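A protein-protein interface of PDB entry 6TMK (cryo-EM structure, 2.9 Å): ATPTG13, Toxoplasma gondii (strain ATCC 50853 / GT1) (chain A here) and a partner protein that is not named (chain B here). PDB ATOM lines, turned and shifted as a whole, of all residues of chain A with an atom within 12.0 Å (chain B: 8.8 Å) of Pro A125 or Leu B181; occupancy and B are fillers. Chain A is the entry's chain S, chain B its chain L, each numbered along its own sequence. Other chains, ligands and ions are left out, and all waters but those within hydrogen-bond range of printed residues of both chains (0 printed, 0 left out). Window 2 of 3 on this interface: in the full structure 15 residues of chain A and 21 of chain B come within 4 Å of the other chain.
Hydrophobic or aromatic side chains of chain B within 4 Å of the printed part of chain A: Val B177 and Leu B181. Printed residues of chain A that touch a printed residue of chain B: Leu A123 and Pro A125. Among the printed residues, 4 pairs touch across the chains.
Of the printed residues of chain B, Leu A123 touches Gln B173 and Ser B174. Of the printed residues of chain B, Pro A125 touches Val B177 and Leu B181. Thr A127 touches none of the printed residues of chain B. Of the printed residues of chain A, Gln B173 touches Leu A123. Of chain A, only Leu A123 (3.3 Å) comes within 4 Å of Ser B174. Ala B175 touches none of the printed residues of chain A. Val B177 touches just one residue of chain A: Pro A125. No residue of chain A comes within 4 Å of Asn B179. No residue of chain A comes within 4 Å of Gln B184. The nearest residue of chain A that does not touch Leu B181 is Thr A127 (4.05 Å).
The side-chain hydroxyl (OG) of Ser B174 lies close to the backbone carbonyl oxygen (O) of Leu A123 (3.4 Å).
Among the printed residues, merely in contact across the chains: Pro A125 with Leu B181 (3.7 Å), Pro A125 with Val B177 (3.8 Å) and Leu A123 with Gln B173 (3.8 Å).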
ATOM      1  N   PRO A 119      13.988   1.935  -9.762  1.00  0.00           N
ATOM      2  CA  PRO A 119      14.595   2.908  -8.852  1.00  0.00           C
ATOM      3  C   PRO A 119      14.654   2.392  -7.425  1.00  0.00           C
ATOM      4  O   PRO A 119      13.753   1.692  -6.955  1.00  0.00           O
ATOM      5  CB  PRO A 119      13.663   4.120  -8.966  1.00  0.00           C
ATOM      6  CG  PRO A 119      12.370   3.549  -9.372  1.00  0.00           C
ATOM      7  CD  PRO A 119      12.704   2.420 -10.290  1.00  0.00           C
ATOM      8  N   LEU A 121      14.540   4.267  -4.609  1.00  0.00           N
ATOM      9  CA  LEU A 121      13.475   4.977  -3.914  1.00  0.00           C
ATOM     10  C   LEU A 121      12.433   5.427  -4.925  1.00  0.00           C
ATOM     11  O   LEU A 121      12.747   6.175  -5.856  1.00  0.00           O
ATOM     12  CB  LEU A 121      14.026   6.177  -3.148  1.00  0.00           C
ATOM     13  CG  LEU A 121      14.732   5.861  -1.840  1.00  0.00           C
ATOM     14  CD1 LEU A 121      15.801   6.885  -1.584  1.00  0.00           C
ATOM     15  CD2 LEU A 121      13.725   5.844  -0.708  1.00  0.00           C
ATOM     16  N   LEU A 122      11.200   4.968  -4.741  1.00  0.00           N
ATOM     17  CA  LEU A 122      10.071   5.417  -5.546  1.00  0.00           C
ATOM     18  C   LEU A 122       9.416   6.585  -4.816  1.00  0.00           C
ATOM     19  O   LEU A 122       8.805   6.404  -3.759  1.00  0.00           O
ATOM     20  CB  LEU A 122       9.094   4.271  -5.781  1.00  0.00           C
ATOM     21  CG  LEU A 122       8.016   4.501  -6.836  1.00  0.00           C
ATOM     22  CD1 LEU A 122       7.691   3.183  -7.507  1.00  0.00           C
ATOM     23  CD2 LEU A 122       6.763   5.125  -6.241  1.00  0.00           C
ATOM     24  N   LEU A 123       9.540   7.783  -5.387  1.00  0.00           N
ATOM     25  CA  LEU A 123       9.167   9.017  -4.708  1.00  0.00           C
ATOM     26  C   LEU A 123       8.064   9.756  -5.448  1.00  0.00           C
ATOM     27  O   LEU A 123       8.176  10.957  -5.706  1.00  0.00           O
ATOM     28  CB  LEU A 123      10.382   9.927  -4.564  1.00  0.00           C
ATOM     29  CG  LEU A 123      11.498   9.408  -3.670  1.00  0.00           C
ATOM     30  CD1 LEU A 123      12.699  10.301  -3.790  1.00  0.00           C
ATOM     31  CD2 LEU A 123      11.027   9.337  -2.238  1.00  0.00           C
ATOM     32  N   GLY A 124       7.003   9.044  -5.799  1.00  0.00           N
ATOM     33  CA  GLY A 124       5.823   9.667  -6.337  1.00  0.00           C
ATOM     34  C   GLY A 124       4.977   8.677  -7.103  1.00  0.00           C
ATOM     35  O   GLY A 124       5.421   7.580  -7.453  1.00  0.00           O
ATOM     36  N   PRO A 125       3.734   9.046  -7.375  1.00  0.00           N
ATOM     37  CA  PRO A 125       2.838   8.156  -8.112  1.00  0.00           C
ATOM     38  C   PRO A 125       3.119   8.186  -9.608  1.00  0.00           C
ATOM     39  O   PRO A 125       3.815   9.056 -10.131  1.00  0.00           O
ATOM     40  CB  PRO A 125       1.451   8.719  -7.797  1.00  0.00           C
ATOM     41  CG  PRO A 125       1.690  10.166  -7.573  1.00  0.00           C
ATOM     42  CD  PRO A 125       3.056  10.281  -6.951  1.00  0.00           C
ATOM     43  N   SER A 126       2.558   7.193 -10.293  1.00  0.00           N
ATOM     44  CA  SER A 126       2.611   7.092 -11.751  1.00  0.00           C
ATOM     45  C   SER A 126       1.212   6.675 -12.193  1.00  0.00           C
ATOM     46  O   SER A 126       0.906   5.484 -12.297  1.00  0.00           O
ATOM     47  CB  SER A 126       3.673   6.103 -12.205  1.00  0.00           C
ATOM     48  OG  SER A 126       4.936   6.421 -11.648  1.00  0.00           O
ATOM     49  N   THR A 127       0.368   7.667 -12.450  1.00  0.00           N
ATOM     50  CA  THR A 127      -1.041   7.430 -12.724  1.00  0.00           C
ATOM     51  C   THR A 127      -1.348   7.597 -14.206  1.00  0.00           C
ATOM     52  O   THR A 127      -1.679   6.630 -14.892  1.00  0.00           O
ATOM     53  CB  THR A 127      -1.927   8.387 -11.909  1.00  0.00           C
ATOM     54  OG1 THR A 127      -1.668   9.738 -12.307  1.00  0.00           O
ATOM     55  CG2 THR A 127      -1.630   8.248 -10.428  1.00  0.00           C
ATOM     56  N   ARG B  52       3.199  22.163 -23.862  1.00  0.00           N
ATOM     57  CA  ARG B  52       3.395  20.741 -23.617  1.00  0.00           C
ATOM     58  C   ARG B  52       4.550  20.198 -24.447  1.00  0.00           C
ATOM     59  O   ARG B  52       5.418  19.480 -23.937  1.00  0.00           O
ATOM     60  CB  ARG B  52       2.091  20.007 -23.929  1.00  0.00           C
ATOM     61  CG  ARG B  52       2.025  18.567 -23.510  1.00  0.00           C
ATOM     62  CD  ARG B  52       1.911  18.419 -22.014  1.00  0.00           C
ATOM     63  NE  ARG B  52       2.067  17.029 -21.603  1.00  0.00           N
ATOM     64  CZ  ARG B  52       1.102  16.269 -21.103  1.00  0.00           C
ATOM     65  NH1 ARG B  52       1.365  15.021 -20.773  1.00  0.00           N
ATOM     66  NH2 ARG B  52      -0.119  16.741 -20.925  1.00  0.00           N
ATOM     67  N   GLN B 173      10.234  16.253  -3.326  1.00  0.00           N
ATOM     68  CA  GLN B 173      10.200  15.569  -4.615  1.00  0.00           C
ATOM     69  C   GLN B 173       8.854  14.888  -4.841  1.00  0.00           C
ATOM     70  O   GLN B 173       8.246  15.010  -5.917  1.00  0.00           O
ATOM     71  CB  GLN B 173      11.344  14.565  -4.684  1.00  0.00           C
ATOM     72  CG  GLN B 173      11.662  14.088  -6.075  1.00  0.00           C
ATOM     73  CD  GLN B 173      13.023  13.455  -6.175  1.00  0.00           C
ATOM     74  OE1 GLN B 173      13.975  13.896  -5.540  1.00  0.00           O
ATOM     75  NE2 GLN B 173      13.127  12.414  -6.976  1.00  0.00           N
ATOM     76  N   SER B 174       8.370  14.168  -3.827  1.00  0.00           N
ATOM     77  CA  SER B 174       7.085  13.487  -3.945  1.00  0.00           C
ATOM     78  C   SER B 174       5.957  14.474  -4.227  1.00  0.00           C
ATOM     79  O   SER B 174       5.132  14.264  -5.131  1.00  0.00           O
ATOM     80  CB  SER B 174       6.805  12.706  -2.665  1.00  0.00           C
ATOM     81  OG  SER B 174       7.848  11.796  -2.391  1.00  0.00           O
ATOM     82  N   ALA B 175       5.902  15.554  -3.450  1.00  0.00           N
ATOM     83  CA  ALA B 175       4.855  16.549  -3.629  1.00  0.00           C
ATOM     84  C   ALA B 175       4.928  17.183  -5.005  1.00  0.00           C
ATOM     85  O   ALA B 175       3.896  17.456  -5.628  1.00  0.00           O
ATOM     86  CB  ALA B 175       4.968  17.616  -2.549  1.00  0.00           C
ATOM     87  N   ALA B 176       6.139  17.428  -5.498  1.00  0.00           N
ATOM     88  CA  ALA B 176       6.281  18.030  -6.813  1.00  0.00           C
ATOM     89  C   ALA B 176       5.720  17.117  -7.885  1.00  0.00           C
ATOM     90  O   ALA B 176       4.991  17.566  -8.777  1.00  0.00           O
ATOM     91  CB  ALA B 176       7.749  18.337  -7.084  1.00  0.00           C
ATOM     92  N   VAL B 177       6.037  15.826  -7.810  1.00  0.00           N
ATOM     93  CA  VAL B 177       5.508  14.888  -8.796  1.00  0.00           C
ATOM     94  C   VAL B 177       3.985  14.885  -8.760  1.00  0.00           C
ATOM     95  O   VAL B 177       3.319  14.982  -9.800  1.00  0.00           O
ATOM     96  CB  VAL B 177       6.079  13.482  -8.556  1.00  0.00           C
ATOM     97  CG1 VAL B 177       5.397  12.478  -9.449  1.00  0.00           C
ATOM     98  CG2 VAL B 177       7.556  13.475  -8.804  1.00  0.00           C
ATOM     99  N   GLU B 178       3.409  14.784  -7.561  1.00  0.00           N
ATOM    100  CA  GLU B 178       1.954  14.716  -7.451  1.00  0.00           C
ATOM    101  C   GLU B 178       1.293  15.970  -8.016  1.00  0.00           C
ATOM    102  O   GLU B 178       0.343  15.890  -8.810  1.00  0.00           O
ATOM    103  CB  GLU B 178       1.558  14.509  -5.992  1.00  0.00           C
ATOM    104  CG  GLU B 178       0.162  13.955  -5.791  1.00  0.00           C
ATOM    105  CD  GLU B 178      -0.887  15.035  -5.590  1.00  0.00           C
ATOM    106  OE1 GLU B 178      -0.554  16.229  -5.736  1.00  0.00           O
ATOM    107  OE2 GLU B 178      -2.047  14.690  -5.285  1.00  0.00           O
ATOM    108  N   ASN B 179       1.788  17.141  -7.619  1.00  0.00           N
ATOM    109  CA  ASN B 179       1.174  18.387  -8.055  1.00  0.00           C
ATOM    110  C   ASN B 179       1.307  18.572  -9.559  1.00  0.00           C
ATOM    111  O   ASN B 179       0.363  19.026 -10.222  1.00  0.00           O
ATOM    112  CB  ASN B 179       1.813  19.552  -7.311  1.00  0.00           C
ATOM    113  CG  ASN B 179       1.591  19.479  -5.822  1.00  0.00           C
ATOM    114  OD1 ASN B 179       0.784  18.686  -5.341  1.00  0.00           O
ATOM    115  ND2 ASN B 179       2.312  20.300  -5.081  1.00  0.00           N
ATOM    116  N   SER B 180       2.471  18.239 -10.116  1.00  0.00           N
ATOM    117  CA  SER B 180       2.651  18.356 -11.556  1.00  0.00           C
ATOM    118  C   SER B 180       1.699  17.435 -12.303  1.00  0.00           C
ATOM    119  O   SER B 180       1.123  17.825 -13.324  1.00  0.00           O
ATOM    120  CB  SER B 180       4.098  18.052 -11.920  1.00  0.00           C
ATOM    121  OG  SER B 180       4.970  18.999 -11.342  1.00  0.00           O
ATOM    122  N   LEU B 181       1.506  16.212 -11.804  1.00  0.00           N
ATOM    123  CA  LEU B 181       0.567  15.299 -12.444  1.00  0.00           C
ATOM    124  C   LEU B 181      -0.841  15.876 -12.444  1.00  0.00           C
ATOM    125  O   LEU B 181      -1.544  15.844 -13.463  1.00  0.00           O
ATOM    126  CB  LEU B 181       0.577  13.955 -11.728  1.00  0.00           C
ATOM    127  CG  LEU B 181       1.662  12.960 -12.108  1.00  0.00           C
ATOM    128  CD1 LEU B 181       1.621  11.800 -11.163  1.00  0.00           C
ATOM    129  CD2 LEU B 181       1.475  12.482 -13.515  1.00  0.00           C
ATOM    130  N   VAL B 182      -1.266  16.412 -11.302  1.00  0.00           N
ATOM    131  CA  VAL B 182      -2.622  16.941 -11.193  1.00  0.00           C
ATOM    132  C   VAL B 182      -2.818  18.106 -12.153  1.00  0.00           C
ATOM    133  O   VAL B 182      -3.815  18.177 -12.889  1.00  0.00           O
ATOM    134  CB  VAL B 182      -2.908  17.348  -9.737  1.00  0.00           C
ATOM    135  CG1 VAL B 182      -4.172  18.157  -9.644  1.00  0.00           C
ATOM    136  CG2 VAL B 182      -3.008  16.123  -8.873  1.00  0.00           C
ATOM    137  N   ARG B 183      -1.865  19.035 -12.162  1.00  0.00           N
ATOM    138  CA  ARG B 183      -1.954  20.196 -13.038  1.00  0.00           C
ATOM    139  C   ARG B 183      -1.996  19.779 -14.504  1.00  0.00           C
ATOM    140  O   ARG B 183      -2.806  20.287 -15.292  1.00  0.00           O
ATOM    141  CB  ARG B 183      -0.765  21.106 -12.761  1.00  0.00           C
ATOM    142  CG  ARG B 183      -0.804  22.439 -13.435  1.00  0.00           C
ATOM    143  CD  ARG B 183       0.078  23.410 -12.702  1.00  0.00           C
ATOM    144  NE  ARG B 183       1.440  22.904 -12.565  1.00  0.00           N
ATOM    145  CZ  ARG B 183       2.071  22.703 -11.408  1.00  0.00           C
ATOM    146  NH1 ARG B 183       1.479  22.950 -10.247  1.00  0.00           N
ATOM    147  NH2 ARG B 183       3.312  22.241 -11.412  1.00  0.00           N
ATOM    148  N   GLN B 184      -1.110  18.861 -14.884  1.00  0.00           N
ATOM    149  CA  GLN B 184      -1.067  18.358 -16.248  1.00  0.00           C
ATOM    150  C   GLN B 184      -2.406  17.764 -16.666  1.00  0.00           C
ATOM    151  O   GLN B 184      -2.918  18.052 -17.756  1.00  0.00           O
ATOM    152  CB  GLN B 184       0.040  17.316 -16.339  1.00  0.00           C
ATOM    153  CG  GLN B 184       0.616  17.094 -17.689  1.00  0.00           C
ATOM    154  CD  GLN B 184       1.627  15.983 -17.689  1.00  0.00           C
ATOM    155  OE1 GLN B 184       1.291  14.819 -17.488  1.00  0.00           O
ATOM    156  NE2 GLN B 184       2.882  16.335 -17.902  1.00  0.00           N
ATOM    157  N   ASN B 185      -2.983  16.914 -15.815  1.00  0.00           N
ATOM    158  CA  ASN B 185      -4.236  16.261 -16.172  1.00  0.00           C
ATOM    159  C   ASN B 185      -5.361  17.274 -16.316  1.00  0.00           C
ATOM    160  O   ASN B 185      -6.183  17.177 -17.237  1.00  0.00           O
ATOM    161  CB  ASN B 185      -4.588  15.202 -15.132  1.00  0.00           C
ATOM    162  CG  ASN B 185      -5.702  14.293 -15.585  1.00  0.00           C
ATOM    163  OD1 ASN B 185      -5.510  13.441 -16.451  1.00  0.00           O
ATOM    164  ND2 ASN B 185      -6.876  14.462 -14.994  1.00  0.00           N
ATOM    165  N   MET B 186      -5.413  18.260 -15.419  1.00  0.00           N
ATOM    166  CA  MET B 186      -6.432  19.297 -15.534  1.00  0.00           C
ATOM    167  C   MET B 186      -6.307  20.036 -16.859  1.00  0.00           C
ATOM    168  O   MET B 186      -7.303  20.263 -17.560  1.00  0.00           O
ATOM    169  CB  MET B 186      -6.321  20.269 -14.366  1.00  0.00           C
ATOM    170  CG  MET B 186      -6.991  19.800 -13.093  1.00  0.00           C
ATOM    171  SD  MET B 186      -7.528  21.178 -12.067  1.00  0.00           S
ATOM    172  CE  MET B 186      -5.974  22.033 -11.826  1.00  0.00           C
ATOM    173  N   ALA B 187      -5.082  20.424 -17.216  1.00  0.00           N
ATOM    174  CA  ALA B 187      -4.875  21.144 -18.466  1.00  0.00           C
ATOM    175  C   ALA B 187      -5.291  20.309 -19.671  1.00  0.00           C
ATOM    176  O   ALA B 187      -5.917  20.821 -20.608  1.00  0.00           O
ATOM    177  CB  ALA B 187      -3.416  21.558 -18.587  1.00  0.00           C
ATOM    178  N   ASP B 188      -4.958  19.020 -19.666  1.00  0.00           N
ATOM    179  CA  ASP B 188      -5.302  18.176 -20.806  1.00  0.00           C
ATOM    180  C   ASP B 188      -6.810  18.001 -20.929  1.00  0.00           C
ATOM    181  O   ASP B 188      -7.355  18.007 -22.041  1.00  0.00           O
ATOM    182  CB  ASP B 188      -4.610  16.826 -20.684  1.00  0.00           C
ATOM    183  CG  ASP B 188      -3.106  16.948 -20.603  1.00  0.00           C
ATOM    184  OD1 ASP B 188      -2.567  17.978 -21.049  1.00  0.00           O
ATOM    185  OD2 ASP B 188      -2.458  16.010 -20.100  1.00  0.00           O
